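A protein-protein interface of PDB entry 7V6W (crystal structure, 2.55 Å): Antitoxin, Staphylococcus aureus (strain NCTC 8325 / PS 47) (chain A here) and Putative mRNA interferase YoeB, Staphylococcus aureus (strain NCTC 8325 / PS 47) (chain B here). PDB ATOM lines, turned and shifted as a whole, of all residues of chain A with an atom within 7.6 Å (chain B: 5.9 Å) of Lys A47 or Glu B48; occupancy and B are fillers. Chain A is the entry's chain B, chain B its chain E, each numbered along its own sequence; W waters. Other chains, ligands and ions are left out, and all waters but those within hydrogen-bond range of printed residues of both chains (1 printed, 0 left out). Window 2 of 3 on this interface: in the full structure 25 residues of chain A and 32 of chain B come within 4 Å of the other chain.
Among the printed residues, merely in contact across the chains: Lys A47 with Glu B48 (3.7 Å), Ser A48 with Lys B49 (3.6 Å), Glu A51 with Leu B50 (3.6 Å) and Thr A52 with Leu B50 (3.6 Å).
Hydrophobic or aromatic side chains of chain B within 4 Å of the printed part of chain A: Leu B50.
Among the printed residues, 7 pairs touch across the chains.
Lys A47 touches just one residue of chain B: Glu B48.
Of the printed residues of chain A, Lys B49 touches Ser A48 (3.6 Å).
Of the printed residues of chain B, Thr A52 touches Leu B50.
Printed residues of chain A within 4 Å of Leu B50: Glu A51 and Thr A52.
Phe B47 touches none of the printed residues of chain A.
The nearest printed residue of chain A that does not touch Lys B53 is Asp A45 (6.3 Å).
OE1 of Glu B48 is in hydrogen-bond range of OG of Ser A48, 2.7 Å away.
NZ of Lys B53 is in hydrogen-bond range of OG of Ser A48 (3.5 Å).
OG of Ser B59 lies within hydrogen-bond range of OE1 of Glu A51 (3.0 Å).
N of Ser B59 is in hydrogen-bond range of O of Glu B48 (3.0 Å).
The side-chain amino group (NZ) of Lys A47 is in salt-bridge range of the side-chain carboxylate (OE1) of Glu A44.
O of Ser A48 sits at hydrogen-bond distance from OG1 of Thr A52, 2.8 Å away.
The backbone carbonyl oxygen (O) of Lys B49 lies within hydrogen-bond range of the side-chain amino group (NZ) of Lys B53, at 3.1 Å.
The backbone NH (N) of Leu B50 lies within hydrogen-bond range of the backbone carbonyl oxygen (O) of Arg B57 (2.8 Å).
Water W1 lies within hydrogen-bond range of the side-chain carboxylate (OE1) of Glu B48 and the backbone carbonyl oxygen (O) of Glu A44.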
ATOM      1  N   ILE A  41     -22.637   7.061   5.617  1.00  0.00           N
ATOM      2  CA  ILE A  41     -22.529   7.561   6.983  1.00  0.00           C
ATOM      3  C   ILE A  41     -22.276   6.385   7.914  1.00  0.00           C
ATOM      4  O   ILE A  41     -22.864   5.311   7.748  1.00  0.00           O
ATOM      5  CB  ILE A  41     -23.800   8.327   7.411  1.00  0.00           C
ATOM      6  CG1 ILE A  41     -24.075   9.482   6.450  1.00  0.00           C
ATOM      7  CG2 ILE A  41     -23.669   8.850   8.833  1.00  0.00           C
ATOM      8  CD1 ILE A  41     -25.454   9.441   5.843  1.00  0.00           C
ATOM      9  N   GLY A  42     -21.393   6.587   8.892  1.00  0.00           N
ATOM     10  CA  GLY A  42     -21.159   5.559   9.887  1.00  0.00           C
ATOM     11  C   GLY A  42     -22.416   5.239  10.673  1.00  0.00           C
ATOM     12  O   GLY A  42     -23.279   6.094  10.887  1.00  0.00           O
ATOM     13  N   LEU A  43     -22.512   3.983  11.111  1.00  0.00           N
ATOM     14  CA  LEU A  43     -23.734   3.511  11.756  1.00  0.00           C
ATOM     15  C   LEU A  43     -23.994   4.243  13.069  1.00  0.00           C
ATOM     16  O   LEU A  43     -25.124   4.664  13.340  1.00  0.00           O
ATOM     17  CB  LEU A  43     -23.654   2.002  11.987  1.00  0.00           C
ATOM     18  CG  LEU A  43     -24.888   1.403  12.659  1.00  0.00           C
ATOM     19  CD1 LEU A  43     -26.123   1.692  11.822  1.00  0.00           C
ATOM     20  CD2 LEU A  43     -24.717  -0.092  12.882  1.00  0.00           C
ATOM     21  N   GLU A  44     -22.961   4.400  13.902  1.00  0.00           N
ATOM     22  CA  GLU A  44     -23.142   5.081  15.182  1.00  0.00           C
ATOM     23  C   GLU A  44     -23.560   6.533  14.982  1.00  0.00           C
ATOM     24  O   GLU A  44     -24.390   7.058  15.733  1.00  0.00           O
ATOM     25  CB  GLU A  44     -21.860   5.000  16.011  1.00  0.00           C
ATOM     26  CG  GLU A  44     -21.787   3.799  16.949  1.00  0.00           C
ATOM     27  CD  GLU A  44     -22.275   2.516  16.306  1.00  0.00           C
ATOM     28  OE1 GLU A  44     -23.366   2.039  16.685  1.00  0.00           O
ATOM     29  OE2 GLU A  44     -21.574   1.990  15.416  1.00  0.00           O
ATOM     30  N   ASP A  45     -22.998   7.200  13.970  1.00  0.00           N
ATOM     31  CA  ASP A  45     -23.411   8.567  13.672  1.00  0.00           C
ATOM     32  C   ASP A  45     -24.824   8.612  13.109  1.00  0.00           C
ATOM     33  O   ASP A  45     -25.571   9.560  13.382  1.00  0.00           O
ATOM     34  CB  ASP A  45     -22.430   9.214  12.693  1.00  0.00           C
ATOM     35  CG  ASP A  45     -21.024   9.310  13.252  1.00  0.00           C
ATOM     36  OD1 ASP A  45     -20.880   9.620  14.454  1.00  0.00           O
ATOM     37  OD2 ASP A  45     -20.063   9.073  12.491  1.00  0.00           O
ATOM     38  N   TRP A  46     -25.211   7.601  12.329  1.00  0.00           N
ATOM     39  CA  TRP A  46     -26.543   7.587  11.734  1.00  0.00           C
ATOM     40  C   TRP A  46     -27.635   7.393  12.780  1.00  0.00           C
ATOM     41  O   TRP A  46     -28.753   7.889  12.601  1.00  0.00           O
ATOM     42  CB  TRP A  46     -26.627   6.493  10.668  1.00  0.00           C
ATOM     43  CG  TRP A  46     -28.028   6.139  10.266  1.00  0.00           C
ATOM     44  CD1 TRP A  46     -28.744   5.046  10.662  1.00  0.00           C
ATOM     45  CD2 TRP A  46     -28.886   6.885   9.393  1.00  0.00           C
ATOM     46  NE1 TRP A  46     -29.991   5.062  10.088  1.00  0.00           N
ATOM     47  CE2 TRP A  46     -30.105   6.181   9.306  1.00  0.00           C
ATOM     48  CE3 TRP A  46     -28.743   8.075   8.676  1.00  0.00           C
ATOM     49  CZ2 TRP A  46     -31.171   6.629   8.529  1.00  0.00           C
ATOM     50  CZ3 TRP A  46     -29.804   8.519   7.907  1.00  0.00           C
ATOM     51  CH2 TRP A  46     -31.002   7.797   7.839  1.00  0.00           C
ATOM     52  N   LYS A  47     -27.337   6.680  13.869  1.00  0.00           N
ATOM     53  CA  LYS A  47     -28.359   6.421  14.879  1.00  0.00           C
ATOM     54  C   LYS A  47     -28.854   7.716  15.513  1.00  0.00           C
ATOM     55  O   LYS A  47     -30.047   7.853  15.810  1.00  0.00           O
ATOM     56  CB  LYS A  47     -27.822   5.463  15.943  1.00  0.00           C
ATOM     57  CG  LYS A  47     -27.540   4.062  15.414  1.00  0.00           C
ATOM     58  CD  LYS A  47     -27.635   3.006  16.506  1.00  0.00           C
ATOM     59  CE  LYS A  47     -26.438   3.041  17.439  1.00  0.00           C
ATOM     60  NZ  LYS A  47     -26.500   1.939  18.442  1.00  0.00           N
ATOM     61  N   SER A  48     -27.955   8.683  15.718  1.00  0.00           N
ATOM     62  CA  SER A  48     -28.373   9.980  16.243  1.00  0.00           C
ATOM     63  C   SER A  48     -29.243  10.727  15.241  1.00  0.00           C
ATOM     64  O   SER A  48     -30.184  11.429  15.627  1.00  0.00           O
ATOM     65  CB  SER A  48     -27.150  10.819  16.614  1.00  0.00           C
ATOM     66  OG  SER A  48     -26.353  10.167  17.586  1.00  0.00           O
ATOM     67  N   ILE A  49     -28.942  10.587  13.948  1.00  0.00           N
ATOM     68  CA  ILE A  49     -29.725  11.267  12.922  1.00  0.00           C
ATOM     69  C   ILE A  49     -31.112  10.646  12.811  1.00  0.00           C
ATOM     70  O   ILE A  49     -32.125  11.353  12.762  1.00  0.00           O
ATOM     71  CB  ILE A  49     -28.981  11.237  11.576  1.00  0.00           C
ATOM     72  CG1 ILE A  49     -27.693  12.059  11.659  1.00  0.00           C
ATOM     73  CG2 ILE A  49     -29.876  11.749  10.463  1.00  0.00           C
ATOM     74  CD1 ILE A  49     -26.866  12.023  10.394  1.00  0.00           C
ATOM     75  N   GLN A  50     -31.177   9.314  12.767  1.00  0.00           N
ATOM     76  CA  GLN A  50     -32.467   8.643  12.655  1.00  0.00           C
ATOM     77  C   GLN A  50     -33.329   8.896  13.885  1.00  0.00           C
ATOM     78  O   GLN A  50     -34.548   9.078  13.771  1.00  0.00           O
ATOM     79  CB  GLN A  50     -32.263   7.145  12.437  1.00  0.00           C
ATOM     80  CG  GLN A  50     -33.525   6.397  12.041  1.00  0.00           C
ATOM     81  CD  GLN A  50     -33.238   4.985  11.570  1.00  0.00           C
ATOM     82  OE1 GLN A  50     -32.602   4.201  12.274  1.00  0.00           O
ATOM     83  NE2 GLN A  50     -33.697   4.659  10.367  1.00  0.00           N
ATOM     84  N   GLU A  51     -32.714   8.915  15.069  1.00  0.00           N
ATOM     85  CA  GLU A  51     -33.458   9.233  16.281  1.00  0.00           C
ATOM     86  C   GLU A  51     -34.024  10.647  16.220  1.00  0.00           C
ATOM     87  O   GLU A  51     -35.185  10.877  16.579  1.00  0.00           O
ATOM     88  CB  GLU A  51     -32.555   9.057  17.502  1.00  0.00           C
ATOM     89  CG  GLU A  51     -33.207   9.403  18.827  1.00  0.00           C
ATOM     90  CD  GLU A  51     -34.378   8.503  19.160  1.00  0.00           C
ATOM     91  OE1 GLU A  51     -35.212   8.907  19.995  1.00  0.00           O
ATOM     92  OE2 GLU A  51     -34.464   7.394  18.589  1.00  0.00           O
ATOM     93  N   THR A  52     -33.221  11.605  15.749  1.00  0.00           N
ATOM     94  CA  THR A  52     -33.691  12.983  15.635  1.00  0.00           C
ATOM     95  C   THR A  52     -34.793  13.108  14.588  1.00  0.00           C
ATOM     96  O   THR A  52     -35.791  13.805  14.811  1.00  0.00           O
ATOM     97  CB  THR A  52     -32.523  13.910  15.293  1.00  0.00           C
ATOM     98  OG1 THR A  52     -31.508  13.799  16.300  1.00  0.00           O
ATOM     99  CG2 THR A  52     -32.993  15.355  15.212  1.00  0.00           C
ATOM    100  N   ILE A  53     -34.631  12.444  13.441  1.00  0.00           N
ATOM    101  CA  ILE A  53     -35.638  12.523  12.386  1.00  0.00           C
ATOM    102  C   ILE A  53     -36.954  11.917  12.853  1.00  0.00           C
ATOM    103  O   ILE A  53     -38.037  12.431  12.544  1.00  0.00           O
ATOM    104  CB  ILE A  53     -35.120  11.847  11.102  1.00  0.00           C
ATOM    105  CG1 ILE A  53     -34.054  12.721  10.447  1.00  0.00           C
ATOM    106  CG2 ILE A  53     -36.258  11.589  10.126  1.00  0.00           C
ATOM    107  CD1 ILE A  53     -34.552  14.106  10.084  1.00  0.00           C
ATOM    108  N   SER B  46     -30.612   2.985  25.149  1.00  0.00           N
ATOM    109  CA  SER B  46     -30.492   3.617  23.835  1.00  0.00           C
ATOM    110  C   SER B  46     -30.266   5.121  23.963  1.00  0.00           C
ATOM    111  O   SER B  46     -30.863   5.923  23.241  1.00  0.00           O
ATOM    112  CB  SER B  46     -31.712   3.317  22.963  1.00  0.00           C
ATOM    113  OG  SER B  46     -31.839   1.923  22.740  1.00  0.00           O
ATOM    114  N   PHE B  47     -29.397   5.504  24.897  1.00  0.00           N
ATOM    115  CA  PHE B  47     -29.056   6.907  25.085  1.00  0.00           C
ATOM    116  C   PHE B  47     -28.472   7.488  23.805  1.00  0.00           C
ATOM    117  O   PHE B  47     -27.620   6.877  23.155  1.00  0.00           O
ATOM    118  CB  PHE B  47     -28.063   7.056  26.240  1.00  0.00           C
ATOM    119  CG  PHE B  47     -27.389   8.396  26.294  1.00  0.00           C
ATOM    120  CD1 PHE B  47     -28.069   9.512  26.756  1.00  0.00           C
ATOM    121  CD2 PHE B  47     -26.070   8.538  25.895  1.00  0.00           C
ATOM    122  CE1 PHE B  47     -27.447  10.744  26.811  1.00  0.00           C
ATOM    123  CE2 PHE B  47     -25.443   9.768  25.947  1.00  0.00           C
ATOM    124  CZ  PHE B  47     -26.132  10.874  26.406  1.00  0.00           C
ATOM    125  N   GLU B  48     -28.938   8.682  23.443  1.00  0.00           N
ATOM    126  CA  GLU B  48     -28.560   9.293  22.180  1.00  0.00           C
ATOM    127  C   GLU B  48     -28.481  10.803  22.354  1.00  0.00           C
ATOM    128  O   GLU B  48     -29.328  11.403  23.021  1.00  0.00           O
ATOM    129  CB  GLU B  48     -29.564   8.936  21.078  1.00  0.00           C
ATOM    130  CG  GLU B  48     -28.980   8.907  19.678  1.00  0.00           C
ATOM    131  CD  GLU B  48     -27.825   7.933  19.552  1.00  0.00           C
ATOM    132  OE1 GLU B  48     -26.660   8.383  19.594  1.00  0.00           O
ATOM    133  OE2 GLU B  48     -28.082   6.717  19.424  1.00  0.00           O
ATOM    134  N   LYS B  49     -27.455  11.405  21.757  1.00  0.00           N
ATOM    135  CA  LYS B  49     -27.322  12.856  21.708  1.00  0.00           C
ATOM    136  C   LYS B  49     -28.010  13.348  20.440  1.00  0.00           C
ATOM    137  O   LYS B  49     -27.537  13.086  19.329  1.00  0.00           O
ATOM    138  CB  LYS B  49     -25.852  13.269  21.731  1.00  0.00           C
ATOM    139  CG  LYS B  49     -25.035  12.630  22.842  1.00  0.00           C
ATOM    140  CD  LYS B  49     -23.565  13.011  22.726  1.00  0.00           C
ATOM    141  CE  LYS B  49     -22.718  12.291  23.764  1.00  0.00           C
ATOM    142  NZ  LYS B  49     -23.105  12.647  25.157  1.00  0.00           N
ATOM    143  N   LEU B  50     -29.125  14.054  20.603  1.00  0.00           N
ATOM    144  CA  LEU B  50     -29.920  14.474  19.460  1.00  0.00           C
ATOM    145  C   LEU B  50     -29.184  15.529  18.637  1.00  0.00           C
ATOM    146  O   LEU B  50     -28.226  16.161  19.091  1.00  0.00           O
ATOM    147  CB  LEU B  50     -31.273  15.016  19.920  1.00  0.00           C
ATOM    148  CG  LEU B  50     -32.122  14.030  20.724  1.00  0.00           C
ATOM    149  CD1 LEU B  50     -33.468  14.636  21.080  1.00  0.00           C
ATOM    150  CD2 LEU B  50     -32.298  12.732  19.953  1.00  0.00           C
ATOM    151  N   LYS B  53     -26.023  18.787  17.636  1.00  0.00           N
ATOM    152  CA  LYS B  53     -25.346  18.431  18.879  1.00  0.00           C
ATOM    153  C   LYS B  53     -25.196  19.620  19.819  1.00  0.00           C
ATOM    154  O   LYS B  53     -25.213  19.444  21.042  1.00  0.00           O
ATOM    155  CB  LYS B  53     -23.974  17.830  18.574  1.00  0.00           C
ATOM    156  CG  LYS B  53     -24.007  16.544  17.763  1.00  0.00           C
ATOM    157  CD  LYS B  53     -24.386  15.348  18.622  1.00  0.00           C
ATOM    158  CE  LYS B  53     -24.260  14.049  17.838  1.00  0.00           C
ATOM    159  NZ  LYS B  53     -24.487  12.852  18.694  1.00  0.00           N
ATOM    160  N   ARG B  57     -29.567  18.344  23.516  1.00  0.00           N
ATOM    161  CA  ARG B  57     -30.762  17.602  23.891  1.00  0.00           C
ATOM    162  C   ARG B  57     -30.477  16.110  23.779  1.00  0.00           C
ATOM    163  O   ARG B  57     -29.807  15.665  22.842  1.00  0.00           O
ATOM    164  CB  ARG B  57     -31.955  17.978  23.010  1.00  0.00           C
ATOM    165  CG  ARG B  57     -32.333  19.452  23.058  1.00  0.00           C
ATOM    166  CD  ARG B  57     -33.748  19.668  22.544  1.00  0.00           C
ATOM    167  NE  ARG B  57     -34.054  21.077  22.308  1.00  0.00           N
ATOM    168  CZ  ARG B  57     -34.004  21.661  21.116  1.00  0.00           C
ATOM    169  NH1 ARG B  57     -33.660  20.958  20.045  1.00  0.00           N
ATOM    170  NH2 ARG B  57     -34.303  22.948  20.990  1.00  0.00           N
ATOM    171  N   TYR B  58     -30.980  15.344  24.738  1.00  0.00           N
ATOM    172  CA  TYR B  58     -30.707  13.919  24.817  1.00  0.00           C
ATOM    173  C   TYR B  58     -32.012  13.133  24.782  1.00  0.00           C
ATOM    174  O   TYR B  58     -33.103  13.679  24.956  1.00  0.00           O
ATOM    175  CB  TYR B  58     -29.909  13.584  26.082  1.00  0.00           C
ATOM    176  CG  TYR B  58     -28.618  14.359  26.200  1.00  0.00           C
ATOM    177  CD1 TYR B  58     -27.466  13.933  25.550  1.00  0.00           C
ATOM    178  CD2 TYR B  58     -28.549  15.517  26.963  1.00  0.00           C
ATOM    179  CE1 TYR B  58     -26.282  14.639  25.658  1.00  0.00           C
ATOM    180  CE2 TYR B  58     -27.371  16.229  27.077  1.00  0.00           C
ATOM    181  CZ  TYR B  58     -26.241  15.787  26.423  1.00  0.00           C
ATOM    182  OH  TYR B  58     -25.067  16.497  26.536  1.00  0.00           O
ATOM    183  N   SER B  59     -31.882  11.828  24.553  1.00  0.00           N
ATOM    184  CA  SER B  59     -33.042  10.969  24.377  1.00  0.00           C
ATOM    185  C   SER B  59     -32.753   9.588  24.942  1.00  0.00           C
ATOM    186  O   SER B  59     -31.657   9.050  24.761  1.00  0.00           O
ATOM    187  CB  SER B  59     -33.426  10.858  22.897  1.00  0.00           C
ATOM    188  OG  SER B  59     -34.471   9.923  22.712  1.00  0.00           O
ATOM    189  N   ARG B  60     -33.744   9.023  25.627  1.00  0.00           N
ATOM    190  CA  ARG B  60     -33.706   7.639  26.073  1.00  0.00           C
ATOM    191  C   ARG B  60     -35.031   6.979  25.726  1.00  0.00           C
ATOM    192  O   ARG B  60     -36.059   7.647  25.602  1.00  0.00           O
ATOM    193  CB  ARG B  60     -33.426   7.535  27.578  1.00  0.00           C
ATOM    194  CG  ARG B  60     -32.007   7.926  27.942  1.00  0.00           C
ATOM    195  CD  ARG B  60     -31.758   7.879  29.435  1.00  0.00           C
ATOM    196  NE  ARG B  60     -30.398   8.308  29.741  1.00  0.00           N
ATOM    197  CZ  ARG B  60     -29.367   7.483  29.872  1.00  0.00           C
ATOM    198  NH1 ARG B  60     -29.540   6.174  29.739  1.00  0.00           N
ATOM    199  NH2 ARG B  60     -28.162   7.963  30.144  1.00  0.00           N
HETATM  200  O   HOH W   1     -25.058   6.625  18.727  1.00  0.00           O
